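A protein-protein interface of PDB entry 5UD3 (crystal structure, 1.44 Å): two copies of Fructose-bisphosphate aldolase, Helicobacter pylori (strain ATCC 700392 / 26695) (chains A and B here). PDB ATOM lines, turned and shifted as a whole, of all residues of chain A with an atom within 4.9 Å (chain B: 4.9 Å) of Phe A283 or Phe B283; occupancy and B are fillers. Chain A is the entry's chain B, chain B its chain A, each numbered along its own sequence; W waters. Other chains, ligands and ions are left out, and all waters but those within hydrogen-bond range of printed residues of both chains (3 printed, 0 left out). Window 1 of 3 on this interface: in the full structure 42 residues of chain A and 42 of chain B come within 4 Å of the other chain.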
ATOM      1  N   ASN A  26     -19.848  -2.198  17.656  1.00  0.00           N
ATOM      2  CA  ASN A  26     -19.321  -0.860  17.396  1.00  0.00           C
ATOM      3  C   ASN A  26     -19.051  -0.140  18.720  1.00  0.00           C
ATOM      4  O   ASN A  26     -19.145  -0.729  19.802  1.00  0.00           O
ATOM      5  CB  ASN A  26     -20.241  -0.092  16.442  1.00  0.00           C
ATOM      6  CG  ASN A  26     -21.574   0.289  17.064  1.00  0.00           C
ATOM      7  OD1 ASN A  26     -21.797   0.129  18.267  1.00  0.00           O
ATOM      8  ND2 ASN A  26     -22.476   0.808  16.230  1.00  0.00           N
ATOM      9  N   GLU A  28     -20.698   2.444  20.207  1.00  0.00           N
ATOM     10  CA  GLU A  28     -21.839   2.744  21.062  1.00  0.00           C
ATOM     11  C   GLU A  28     -22.227   1.549  21.919  1.00  0.00           C
ATOM     12  O   GLU A  28     -22.517   1.708  23.110  1.00  0.00           O
ATOM     13  CB  GLU A  28     -23.019   3.207  20.221  1.00  0.00           C
ATOM     14  CG  GLU A  28     -22.927   4.663  19.806  1.00  0.00           C
ATOM     15  CD  GLU A  28     -22.148   4.892  18.535  1.00  0.00           C
ATOM     16  OE1 GLU A  28     -21.640   3.916  17.933  1.00  0.00           O
ATOM     17  OE2 GLU A  28     -22.073   6.071  18.133  1.00  0.00           O
ATOM     18  N   TYR A  55     -17.011  -6.886  10.521  1.00  0.00           N
ATOM     19  CA  TYR A  55     -17.588  -5.548  10.415  1.00  0.00           C
ATOM     20  C   TYR A  55     -16.628  -4.481  10.937  1.00  0.00           C
ATOM     21  O   TYR A  55     -16.397  -3.461  10.275  1.00  0.00           O
ATOM     22  CB  TYR A  55     -18.895  -5.546  11.209  1.00  0.00           C
ATOM     23  CG  TYR A  55     -19.622  -4.233  11.242  1.00  0.00           C
ATOM     24  CD1 TYR A  55     -20.401  -3.817  10.170  1.00  0.00           C
ATOM     25  CD2 TYR A  55     -19.540  -3.407  12.356  1.00  0.00           C
ATOM     26  CE1 TYR A  55     -21.071  -2.607  10.205  1.00  0.00           C
ATOM     27  CE2 TYR A  55     -20.202  -2.218  12.406  1.00  0.00           C
ATOM     28  CZ  TYR A  55     -20.972  -1.811  11.327  1.00  0.00           C
ATOM     29  OH  TYR A  55     -21.638  -0.606  11.381  1.00  0.00           O
ATOM     30  N   PHE A 262     -31.493  -0.967  21.854  1.00  0.00           N
ATOM     31  CA  PHE A 262     -30.786   0.075  21.119  1.00  0.00           C
ATOM     32  C   PHE A 262     -31.608   0.548  19.929  1.00  0.00           C
ATOM     33  O   PHE A 262     -31.857   1.751  19.767  1.00  0.00           O
ATOM     34  CB  PHE A 262     -29.455  -0.503  20.649  1.00  0.00           C
ATOM     35  CG  PHE A 262     -28.511   0.506  20.074  1.00  0.00           C
ATOM     36  CD1 PHE A 262     -27.516   1.065  20.859  1.00  0.00           C
ATOM     37  CD2 PHE A 262     -28.591   0.874  18.743  1.00  0.00           C
ATOM     38  CE1 PHE A 262     -26.640   1.993  20.327  1.00  0.00           C
ATOM     39  CE2 PHE A 262     -27.711   1.798  18.207  1.00  0.00           C
ATOM     40  CZ  PHE A 262     -26.742   2.355  18.999  1.00  0.00           C
ATOM     41  N   VAL A 266     -33.436   4.180  18.361  1.00  0.00           N
ATOM     42  CA  VAL A 266     -33.137   4.728  17.037  1.00  0.00           C
ATOM     43  C   VAL A 266     -34.427   4.943  16.252  1.00  0.00           C
ATOM     44  O   VAL A 266     -34.628   5.994  15.623  1.00  0.00           O
ATOM     45  CB  VAL A 266     -32.156   3.800  16.289  1.00  0.00           C
ATOM     46  CG1 VAL A 266     -31.967   4.230  14.813  1.00  0.00           C
ATOM     47  CG2 VAL A 266     -30.817   3.707  17.034  1.00  0.00           C
ATOM     48  N   LEU A 279     -26.114  12.095  14.368  1.00  0.00           N
ATOM     49  CA  LEU A 279     -26.028  10.707  14.824  1.00  0.00           C
ATOM     50  C   LEU A 279     -26.113  10.610  16.343  1.00  0.00           C
ATOM     51  O   LEU A 279     -26.704   9.664  16.883  1.00  0.00           O
ATOM     52  CB  LEU A 279     -24.733  10.047  14.333  1.00  0.00           C
ATOM     53  CG  LEU A 279     -24.685   9.494  12.902  1.00  0.00           C
ATOM     54  CD1 LEU A 279     -24.848  10.602  11.865  1.00  0.00           C
ATOM     55  CD2 LEU A 279     -23.386   8.750  12.683  1.00  0.00           C
ATOM     56  N   ARG A 280     -25.532  11.577  17.054  1.00  0.00           N
ATOM     57  CA  ARG A 280     -25.504  11.507  18.510  1.00  0.00           C
ATOM     58  C   ARG A 280     -26.903  11.587  19.103  1.00  0.00           C
ATOM     59  O   ARG A 280     -27.157  11.033  20.181  1.00  0.00           O
ATOM     60  CB  ARG A 280     -24.632  12.633  19.056  1.00  0.00           C
ATOM     61  CG  ARG A 280     -23.174  12.522  18.644  1.00  0.00           C
ATOM     62  CD  ARG A 280     -22.446  13.853  18.803  1.00  0.00           C
ATOM     63  NE  ARG A 280     -22.939  14.847  17.848  1.00  0.00           N
ATOM     64  CZ  ARG A 280     -22.279  15.945  17.474  1.00  0.00           C
ATOM     65  NH1 ARG A 280     -21.079  16.217  17.959  1.00  0.00           N
ATOM     66  NH2 ARG A 280     -22.830  16.773  16.600  1.00  0.00           N
ATOM     67  N   LYS A 281     -27.819  12.272  18.424  1.00  0.00           N
ATOM     68  CA  LYS A 281     -29.186  12.372  18.917  1.00  0.00           C
ATOM     69  C   LYS A 281     -29.938  11.055  18.780  1.00  0.00           C
ATOM     70  O   LYS A 281     -30.891  10.813  19.530  1.00  0.00           O
ATOM     71  CB  LYS A 281     -29.932  13.467  18.159  1.00  0.00           C
ATOM     72  CG  LYS A 281     -29.362  14.853  18.348  1.00  0.00           C
ATOM     73  CD  LYS A 281     -29.655  15.392  19.724  1.00  0.00           C
ATOM     74  CE  LYS A 281     -29.331  16.874  19.779  1.00  0.00           C
ATOM     75  NZ  LYS A 281     -29.368  17.393  21.173  1.00  0.00           N
ATOM     76  N   PHE A 282     -29.555  10.213  17.818  1.00  0.00           N
ATOM     77  CA  PHE A 282     -30.117   8.866  17.742  1.00  0.00           C
ATOM     78  C   PHE A 282     -29.452   7.934  18.739  1.00  0.00           C
ATOM     79  O   PHE A 282     -30.120   7.099  19.361  1.00  0.00           O
ATOM     80  CB  PHE A 282     -29.910   8.262  16.348  1.00  0.00           C
ATOM     81  CG  PHE A 282     -30.737   8.899  15.266  1.00  0.00           C
ATOM     82  CD1 PHE A 282     -30.325  10.080  14.665  1.00  0.00           C
ATOM     83  CD2 PHE A 282     -31.914   8.315  14.841  1.00  0.00           C
ATOM     84  CE1 PHE A 282     -31.073  10.663  13.666  1.00  0.00           C
ATOM     85  CE2 PHE A 282     -32.673   8.898  13.839  1.00  0.00           C
ATOM     86  CZ  PHE A 282     -32.248  10.076  13.253  1.00  0.00           C
ATOM     87  N   PHE A 283     -28.135   8.039  18.886  1.00  0.00           N
ATOM     88  CA  PHE A 283     -27.393   6.980  19.552  1.00  0.00           C
ATOM     89  C   PHE A 283     -27.155   7.225  21.034  1.00  0.00           C
ATOM     90  O   PHE A 283     -26.834   6.263  21.746  1.00  0.00           O
ATOM     91  CB  PHE A 283     -26.077   6.693  18.828  1.00  0.00           C
ATOM     92  CG  PHE A 283     -26.255   6.328  17.378  1.00  0.00           C
ATOM     93  CD1 PHE A 283     -27.360   5.607  16.958  1.00  0.00           C
ATOM     94  CD2 PHE A 283     -25.326   6.730  16.433  1.00  0.00           C
ATOM     95  CE1 PHE A 283     -27.525   5.282  15.621  1.00  0.00           C
ATOM     96  CE2 PHE A 283     -25.489   6.422  15.100  1.00  0.00           C
ATOM     97  CZ  PHE A 283     -26.586   5.699  14.690  1.00  0.00           C
ATOM     98  N   SER A 284     -27.304   8.467  21.523  1.00  0.00           N
ATOM     99  CA  SER A 284     -27.251   8.673  22.971  1.00  0.00           C
ATOM    100  C   SER A 284     -28.417   7.997  23.682  1.00  0.00           C
ATOM    101  O   SER A 284     -28.179   7.252  24.650  1.00  0.00           O
ATOM    102  CB  SER A 284     -27.145  10.161  23.306  1.00  0.00           C
ATOM    103  OG  SER A 284     -25.874  10.668  22.925  1.00  0.00           O
ATOM    104  N   PRO A 285     -29.672   8.186  23.275  1.00  0.00           N
ATOM    105  CA  PRO A 285     -30.750   7.440  23.942  1.00  0.00           C
ATOM    106  C   PRO A 285     -30.645   5.947  23.720  1.00  0.00           C
ATOM    107  O   PRO A 285     -31.007   5.170  24.613  1.00  0.00           O
ATOM    108  CB  PRO A 285     -32.028   8.032  23.331  1.00  0.00           C
ATOM    109  CG  PRO A 285     -31.592   8.669  22.059  1.00  0.00           C
ATOM    110  CD  PRO A 285     -30.193   9.143  22.281  1.00  0.00           C
ATOM    111  N   ALA A 286     -30.130   5.528  22.563  1.00  0.00           N
ATOM    112  CA  ALA A 286     -29.940   4.109  22.291  1.00  0.00           C
ATOM    113  C   ALA A 286     -28.919   3.487  23.243  1.00  0.00           C
ATOM    114  O   ALA A 286     -29.146   2.393  23.783  1.00  0.00           O
ATOM    115  CB  ALA A 286     -29.519   3.946  20.837  1.00  0.00           C
ATOM    116  N   GLN A 287     -27.792   4.174  23.464  1.00  0.00           N
ATOM    117  CA  GLN A 287     -26.823   3.733  24.465  1.00  0.00           C
ATOM    118  C   GLN A 287     -27.466   3.618  25.843  1.00  0.00           C
ATOM    119  O   GLN A 287     -27.232   2.647  26.570  1.00  0.00           O
ATOM    120  CB  GLN A 287     -25.655   4.711  24.539  1.00  0.00           C
ATOM    121  CG  GLN A 287     -24.633   4.586  23.440  1.00  0.00           C
ATOM    122  CD  GLN A 287     -23.438   5.466  23.740  1.00  0.00           C
ATOM    123  OE1 GLN A 287     -22.776   5.276  24.760  1.00  0.00           O
ATOM    124  NE2 GLN A 287     -23.188   6.469  22.891  1.00  0.00           N
ATOM    125  N   ASN B  26     -18.105   8.660  15.524  1.00  0.00           N
ATOM    126  CA  ASN B  26     -18.078   7.258  15.947  1.00  0.00           C
ATOM    127  C   ASN B  26     -17.318   6.432  14.912  1.00  0.00           C
ATOM    128  O   ASN B  26     -16.751   6.975  13.954  1.00  0.00           O
ATOM    129  CB  ASN B  26     -19.490   6.742  16.231  1.00  0.00           C
ATOM    130  CG  ASN B  26     -20.334   6.573  14.978  1.00  0.00           C
ATOM    131  OD1 ASN B  26     -19.854   6.700  13.840  1.00  0.00           O
ATOM    132  ND2 ASN B  26     -21.614   6.264  15.186  1.00  0.00           N
ATOM    133  N   GLU B  28     -18.374   4.115  12.644  1.00  0.00           N
ATOM    134  CA  GLU B  28     -18.924   3.976  11.297  1.00  0.00           C
ATOM    135  C   GLU B  28     -18.567   5.168  10.418  1.00  0.00           C
ATOM    136  O   GLU B  28     -18.210   4.999   9.246  1.00  0.00           O
ATOM    137  CB  GLU B  28     -20.436   3.791  11.351  1.00  0.00           C
ATOM    138  CG  GLU B  28     -20.864   2.375  11.701  1.00  0.00           C
ATOM    139  CD  GLU B  28     -20.905   2.087  13.174  1.00  0.00           C
ATOM    140  OE1 GLU B  28     -20.611   2.992  13.986  1.00  0.00           O
ATOM    141  OE2 GLU B  28     -21.263   0.941  13.510  1.00  0.00           O
ATOM    142  N   TYR B  55     -18.680  13.112  23.310  1.00  0.00           N
ATOM    143  CA  TYR B  55     -19.468  11.913  23.035  1.00  0.00           C
ATOM    144  C   TYR B  55     -18.592  10.666  23.034  1.00  0.00           C
ATOM    145  O   TYR B  55     -18.935   9.656  23.656  1.00  0.00           O
ATOM    146  CB  TYR B  55     -20.166  12.105  21.688  1.00  0.00           C
ATOM    147  CG  TYR B  55     -20.988  10.935  21.199  1.00  0.00           C
ATOM    148  CD1 TYR B  55     -22.277  10.729  21.660  1.00  0.00           C
ATOM    149  CD2 TYR B  55     -20.478  10.044  20.268  1.00  0.00           C
ATOM    150  CE1 TYR B  55     -23.033   9.665  21.216  1.00  0.00           C
ATOM    151  CE2 TYR B  55     -21.227   8.987  19.816  1.00  0.00           C
ATOM    152  CZ  TYR B  55     -22.509   8.804  20.288  1.00  0.00           C
ATOM    153  OH  TYR B  55     -23.265   7.744  19.843  1.00  0.00           O
ATOM    154  N   PHE B 262     -25.791   9.390   5.752  1.00  0.00           N
ATOM    155  CA  PHE B 262     -25.781   8.274   6.694  1.00  0.00           C
ATOM    156  C   PHE B 262     -27.177   8.016   7.249  1.00  0.00           C
ATOM    157  O   PHE B 262     -27.684   6.888   7.191  1.00  0.00           O
ATOM    158  CB  PHE B 262     -24.816   8.631   7.826  1.00  0.00           C
ATOM    159  CG  PHE B 262     -24.517   7.494   8.761  1.00  0.00           C
ATOM    160  CD1 PHE B 262     -23.380   6.718   8.586  1.00  0.00           C
ATOM    161  CD2 PHE B 262     -25.355   7.211   9.827  1.00  0.00           C
ATOM    162  CE1 PHE B 262     -23.101   5.661   9.443  1.00  0.00           C
ATOM    163  CE2 PHE B 262     -25.077   6.152  10.692  1.00  0.00           C
ATOM    164  CZ  PHE B 262     -23.945   5.383  10.500  1.00  0.00           C
ATOM    165  N   VAL B 266     -30.195   4.870   7.442  1.00  0.00           N
ATOM    166  CA  VAL B 266     -30.747   4.348   8.691  1.00  0.00           C
ATOM    167  C   VAL B 266     -32.269   4.429   8.663  1.00  0.00           C
ATOM    168  O   VAL B 266     -32.969   3.461   8.987  1.00  0.00           O
ATOM    169  CB  VAL B 266     -30.153   5.107   9.895  1.00  0.00           C
ATOM    170  CG1 VAL B 266     -30.835   4.677  11.205  1.00  0.00           C
ATOM    171  CG2 VAL B 266     -28.635   4.922   9.962  1.00  0.00           C
ATOM    172  N   LEU B 279     -27.766  -4.014  14.245  1.00  0.00           N
ATOM    173  CA  LEU B 279     -27.182  -2.695  13.997  1.00  0.00           C
ATOM    174  C   LEU B 279     -26.424  -2.656  12.674  1.00  0.00           C
ATOM    175  O   LEU B 279     -26.438  -1.637  11.972  1.00  0.00           O
ATOM    176  CB  LEU B 279     -26.248  -2.312  15.151  1.00  0.00           C
ATOM    177  CG  LEU B 279     -26.855  -1.685  16.415  1.00  0.00           C
ATOM    178  CD1 LEU B 279     -27.735  -2.664  17.185  1.00  0.00           C
ATOM    179  CD2 LEU B 279     -25.747  -1.141  17.321  1.00  0.00           C
ATOM    180  N   ARG B 280     -25.760  -3.752  12.312  1.00  0.00           N
ATOM    181  CA  ARG B 280     -24.948  -3.760  11.100  1.00  0.00           C
ATOM    182  C   ARG B 280     -25.801  -3.632   9.845  1.00  0.00           C
ATOM    183  O   ARG B 280     -25.330  -3.100   8.832  1.00  0.00           O
ATOM    184  CB  ARG B 280     -24.107  -5.031  11.027  1.00  0.00           C
ATOM    185  CG  ARG B 280     -23.132  -5.197  12.188  1.00  0.00           C
ATOM    186  CD  ARG B 280     -22.687  -6.647  12.346  1.00  0.00           C
ATOM    187  NE  ARG B 280     -23.785  -7.477  12.847  1.00  0.00           N
ATOM    188  CZ  ARG B 280     -23.636  -8.662  13.433  1.00  0.00           C
ATOM    189  NH1 ARG B 280     -22.425  -9.185  13.620  1.00  0.00           N
ATOM    190  NH2 ARG B 280     -24.708  -9.320  13.848  1.00  0.00           N
ATOM    191  N   LYS B 281     -27.047  -4.109   9.890  1.00  0.00           N
ATOM    192  CA  LYS B 281     -27.933  -3.988   8.739  1.00  0.00           C
ATOM    193  C   LYS B 281     -28.388  -2.550   8.524  1.00  0.00           C
ATOM    194  O   LYS B 281     -28.734  -2.178   7.399  1.00  0.00           O
ATOM    195  CB  LYS B 281     -29.139  -4.903   8.929  1.00  0.00           C
ATOM    196  CG  LYS B 281     -28.778  -6.370   8.971  1.00  0.00           C
ATOM    197  CD  LYS B 281     -28.560  -6.930   7.592  1.00  0.00           C
ATOM    198  CE  LYS B 281     -28.302  -8.424   7.672  1.00  0.00           C
ATOM    199  NZ  LYS B 281     -28.238  -9.047   6.324  1.00  0.00           N
ATOM    200  N   PHE B 282     -28.419  -1.741   9.585  1.00  0.00           N
ATOM    201  CA  PHE B 282     -28.661  -0.307   9.456  1.00  0.00           C
ATOM    202  C   PHE B 282     -27.409   0.426   9.008  1.00  0.00           C
ATOM    203  O   PHE B 282     -27.473   1.302   8.141  1.00  0.00           O
ATOM    204  CB  PHE B 282     -29.081   0.283  10.800  1.00  0.00           C
ATOM    205  CG  PHE B 282     -30.454  -0.114  11.240  1.00  0.00           C
ATOM    206  CD1 PHE B 282     -30.676  -1.325  11.891  1.00  0.00           C
ATOM    207  CD2 PHE B 282     -31.527   0.721  11.015  1.00  0.00           C
ATOM    208  CE1 PHE B 282     -31.950  -1.683  12.303  1.00  0.00           C
ATOM    209  CE2 PHE B 282     -32.788   0.374  11.420  1.00  0.00           C
ATOM    210  CZ  PHE B 282     -33.007  -0.839  12.064  1.00  0.00           C
ATOM    211  N   PHE B 283     -26.263   0.079   9.582  1.00  0.00           N
ATOM    212  CA  PHE B 283     -25.091   0.930   9.459  1.00  0.00           C
ATOM    213  C   PHE B 283     -24.166   0.563   8.307  1.00  0.00           C
ATOM    214  O   PHE B 283     -23.358   1.408   7.901  1.00  0.00           O
ATOM    215  CB  PHE B 283     -24.332   0.979  10.785  1.00  0.00           C
ATOM    216  CG  PHE B 283     -25.165   1.467  11.934  1.00  0.00           C
ATOM    217  CD1 PHE B 283     -26.192   2.372  11.731  1.00  0.00           C
ATOM    218  CD2 PHE B 283     -24.941   1.000  13.216  1.00  0.00           C
ATOM    219  CE1 PHE B 283     -26.965   2.805  12.782  1.00  0.00           C
ATOM    220  CE2 PHE B 283     -25.713   1.423  14.266  1.00  0.00           C
ATOM    221  CZ  PHE B 283     -26.726   2.322  14.058  1.00  0.00           C
ATOM    222  N   SER B 284     -24.254  -0.650   7.750  1.00  0.00           N
ATOM    223  CA  SER B 284     -23.475  -0.933   6.545  1.00  0.00           C
ATOM    224  C   SER B 284     -23.948  -0.094   5.363  1.00  0.00           C
ATOM    225  O   SER B 284     -23.104   0.548   4.711  1.00  0.00           O
ATOM    226  CB  SER B 284     -23.460  -2.435   6.251  1.00  0.00           C
ATOM    227  OG  SER B 284     -22.689  -3.130   7.218  1.00  0.00           O
ATOM    228  N   PRO B 285     -25.246  -0.020   5.042  1.00  0.00           N
ATOM    229  CA  PRO B 285     -25.655   0.884   3.954  1.00  0.00           C
ATOM    230  C   PRO B 285     -25.416   2.342   4.278  1.00  0.00           C
ATOM    231  O   PRO B 285     -25.116   3.130   3.373  1.00  0.00           O
ATOM    232  CB  PRO B 285     -27.145   0.579   3.759  1.00  0.00           C
ATOM    233  CG  PRO B 285     -27.583  -0.121   5.005  1.00  0.00           C
ATOM    234  CD  PRO B 285     -26.377  -0.816   5.562  1.00  0.00           C
ATOM    235  N   ALA B 286     -25.515   2.720   5.551  1.00  0.00           N
ATOM    236  CA  ALA B 286     -25.233   4.097   5.942  1.00  0.00           C
ATOM    237  C   ALA B 286     -23.771   4.458   5.685  1.00  0.00           C
ATOM    238  O   ALA B 286     -23.466   5.534   5.156  1.00  0.00           O
ATOM    239  CB  ALA B 286     -25.595   4.286   7.411  1.00  0.00           C
ATOM    240  N   GLN B 287     -22.850   3.572   6.067  1.00  0.00           N
ATOM    241  CA  GLN B 287     -21.438   3.773   5.752  1.00  0.00           C
ATOM    242  C   GLN B 287     -21.225   3.945   4.254  1.00  0.00           C
ATOM    243  O   GLN B 287     -20.493   4.841   3.819  1.00  0.00           O
ATOM    244  CB  GLN B 287     -20.611   2.587   6.237  1.00  0.00           C
ATOM    245  CG  GLN B 287     -20.302   2.548   7.720  1.00  0.00           C
ATOM    246  CD  GLN B 287     -19.314   1.454   8.041  1.00  0.00           C
ATOM    247  OE1 GLN B 287     -18.185   1.483   7.562  1.00  0.00           O
ATOM    248  NE2 GLN B 287     -19.738   0.466   8.830  1.00  0.00           N
HETATM  249  O   HOH W   1     -19.531   3.277  16.452  1.00  0.00           O
HETATM  250  O   HOH W   2     -21.423   8.504  24.285  1.00  0.00           O
HETATM  251  O   HOH W   3     -17.889  -1.877   8.530  1.00  0.00           O
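Water W1 bridges the side-chain carboxylate (OE1) of Glu A28 (2.7 Å) and the side-chain carboxylate (OE1) of Glu B28 (2.7 Å).
Water W3 lies within hydrogen-bond range of O of Tyr A55 (2.8 Å) and NE2 of Gln B287 (3.0 Å).
Water W2 bridges O of Tyr B55 and NE2 of Gln A287.
The side-chain amide nitrogen of Asn B26 lies within hydrogen-bond range of the side-chain carboxylate of Glu A28 (3.0 Å).
ND2 of Asn A26 lies within hydrogen-bond range of OE2 of Glu B28, 3.0 Å away.
OE2 of Glu B28 is in hydrogen-bond range of OH of Tyr A55 (2.7 Å).
The side-chain carboxylate (OE2) of Glu A28 is in hydrogen-bond range of the side-chain hydroxyl (OH) of Tyr B55 (2.7 Å).
The side-chain hydroxyl (OH) of Tyr B55 is in hydrogen-bond range of the side-chain amide nitrogen (NE2) of Gln A287 (3.3 Å).
The side-chain amide nitrogen (NE2) of Gln B287 lies within hydrogen-bond range of the side-chain hydroxyl (OH) of Tyr A55 (3.4 Å).
Of the 14 printed residues of chain A, 10 touch a printed residue of chain B.
Printed residues of chain A that touch a printed residue of chain B: Asn A26, Glu A28, Tyr A55, Phe A262, Val A266, Leu A279, Arg A280, Phe A283, Ser A284 and Gln A287.
Hydrophobic or aromatic side chains of chain A within 4 Å of the printed part of chain B: Tyr A55, Phe A262, Val A266, Leu A279 and Phe A283.
Along chain B the printed residues that touch a printed residue of chain A span positions 26 to 287.
Among the printed residues, 20 pairs touch across the chains.
Among the printed residues, no Asp or Glu carboxylate lies within 4 Å of a Lys or Arg side-chain nitrogen of the other chain.
Asn A26 touches Phe B283, and with the chains exchanged Phe A283 touches Asn B26.
Tyr A55 touches Arg B280, and with the chains exchanged Arg A280 touches Tyr B55.
Tyr A55 touches Gln B287, and with the chains exchanged Gln A287 touches Tyr B55.
Phe B283 touches its own counterpart, Phe A283.
The backbone NH (N) of Glu B28 is in hydrogen-bond range of the side-chain amide oxygen (OD1) of Asn B26, at 3.2 Å.
O of Arg B280 lies within hydrogen-bond range of OG of Ser B284, at 3.1 Å.
The side-chain amide oxygen (OD1) of Asn A26 is in hydrogen-bond range of the backbone NH (N) of Glu A28, 3.2 Å away.
O of Arg A280 is in hydrogen-bond range of OG of Ser A284.
ND2 of Asn A26 touches CE2 of Phe B283, 3.8 Å away.
Tyr A55 touches Arg B280.
CE1 of Tyr A55 touches OG of Ser B284, 3.4 Å away.
CE2 of Phe A262 touches CD2 of Leu B279, 3.6 Å away.
Val B266 touches Val A266.
Asn B26 touches Leu A279 (ND2 to CD2, 3.9 Å).
CD1 of Tyr B55 touches CG of Arg A280 (3.6 Å).
Phe A283 touches Asn B26.
Phe A283 touches Tyr B55 (CB to OH, 3.2 Å).
CE1 of Tyr B55 touches OG of Ser A284, 3.5 Å away.
Of chain A, only Asn A26, Tyr A55 and Phe A283 come within 4 Å of Phe B283.
Printed residues of chain A within 4 Å of Arg B280: Tyr A55 (3.7 Å).
Of the printed residues of chain B, Tyr A55 touches Glu B28 (2.7 Å), Arg B280 (3.7 Å), Phe B283 (3.2 Å), Ser B284 (3.4 Å) and Gln B287 (3.4 Å).
Phe A282 touches none of the printed residues of chain B.
The nearest residue of chain B that does not touch Phe A283 is Phe B262 (4.3 Å).
The nearest residue of chain A that does not touch Phe B283 is Phe A262 (4.3 Å).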
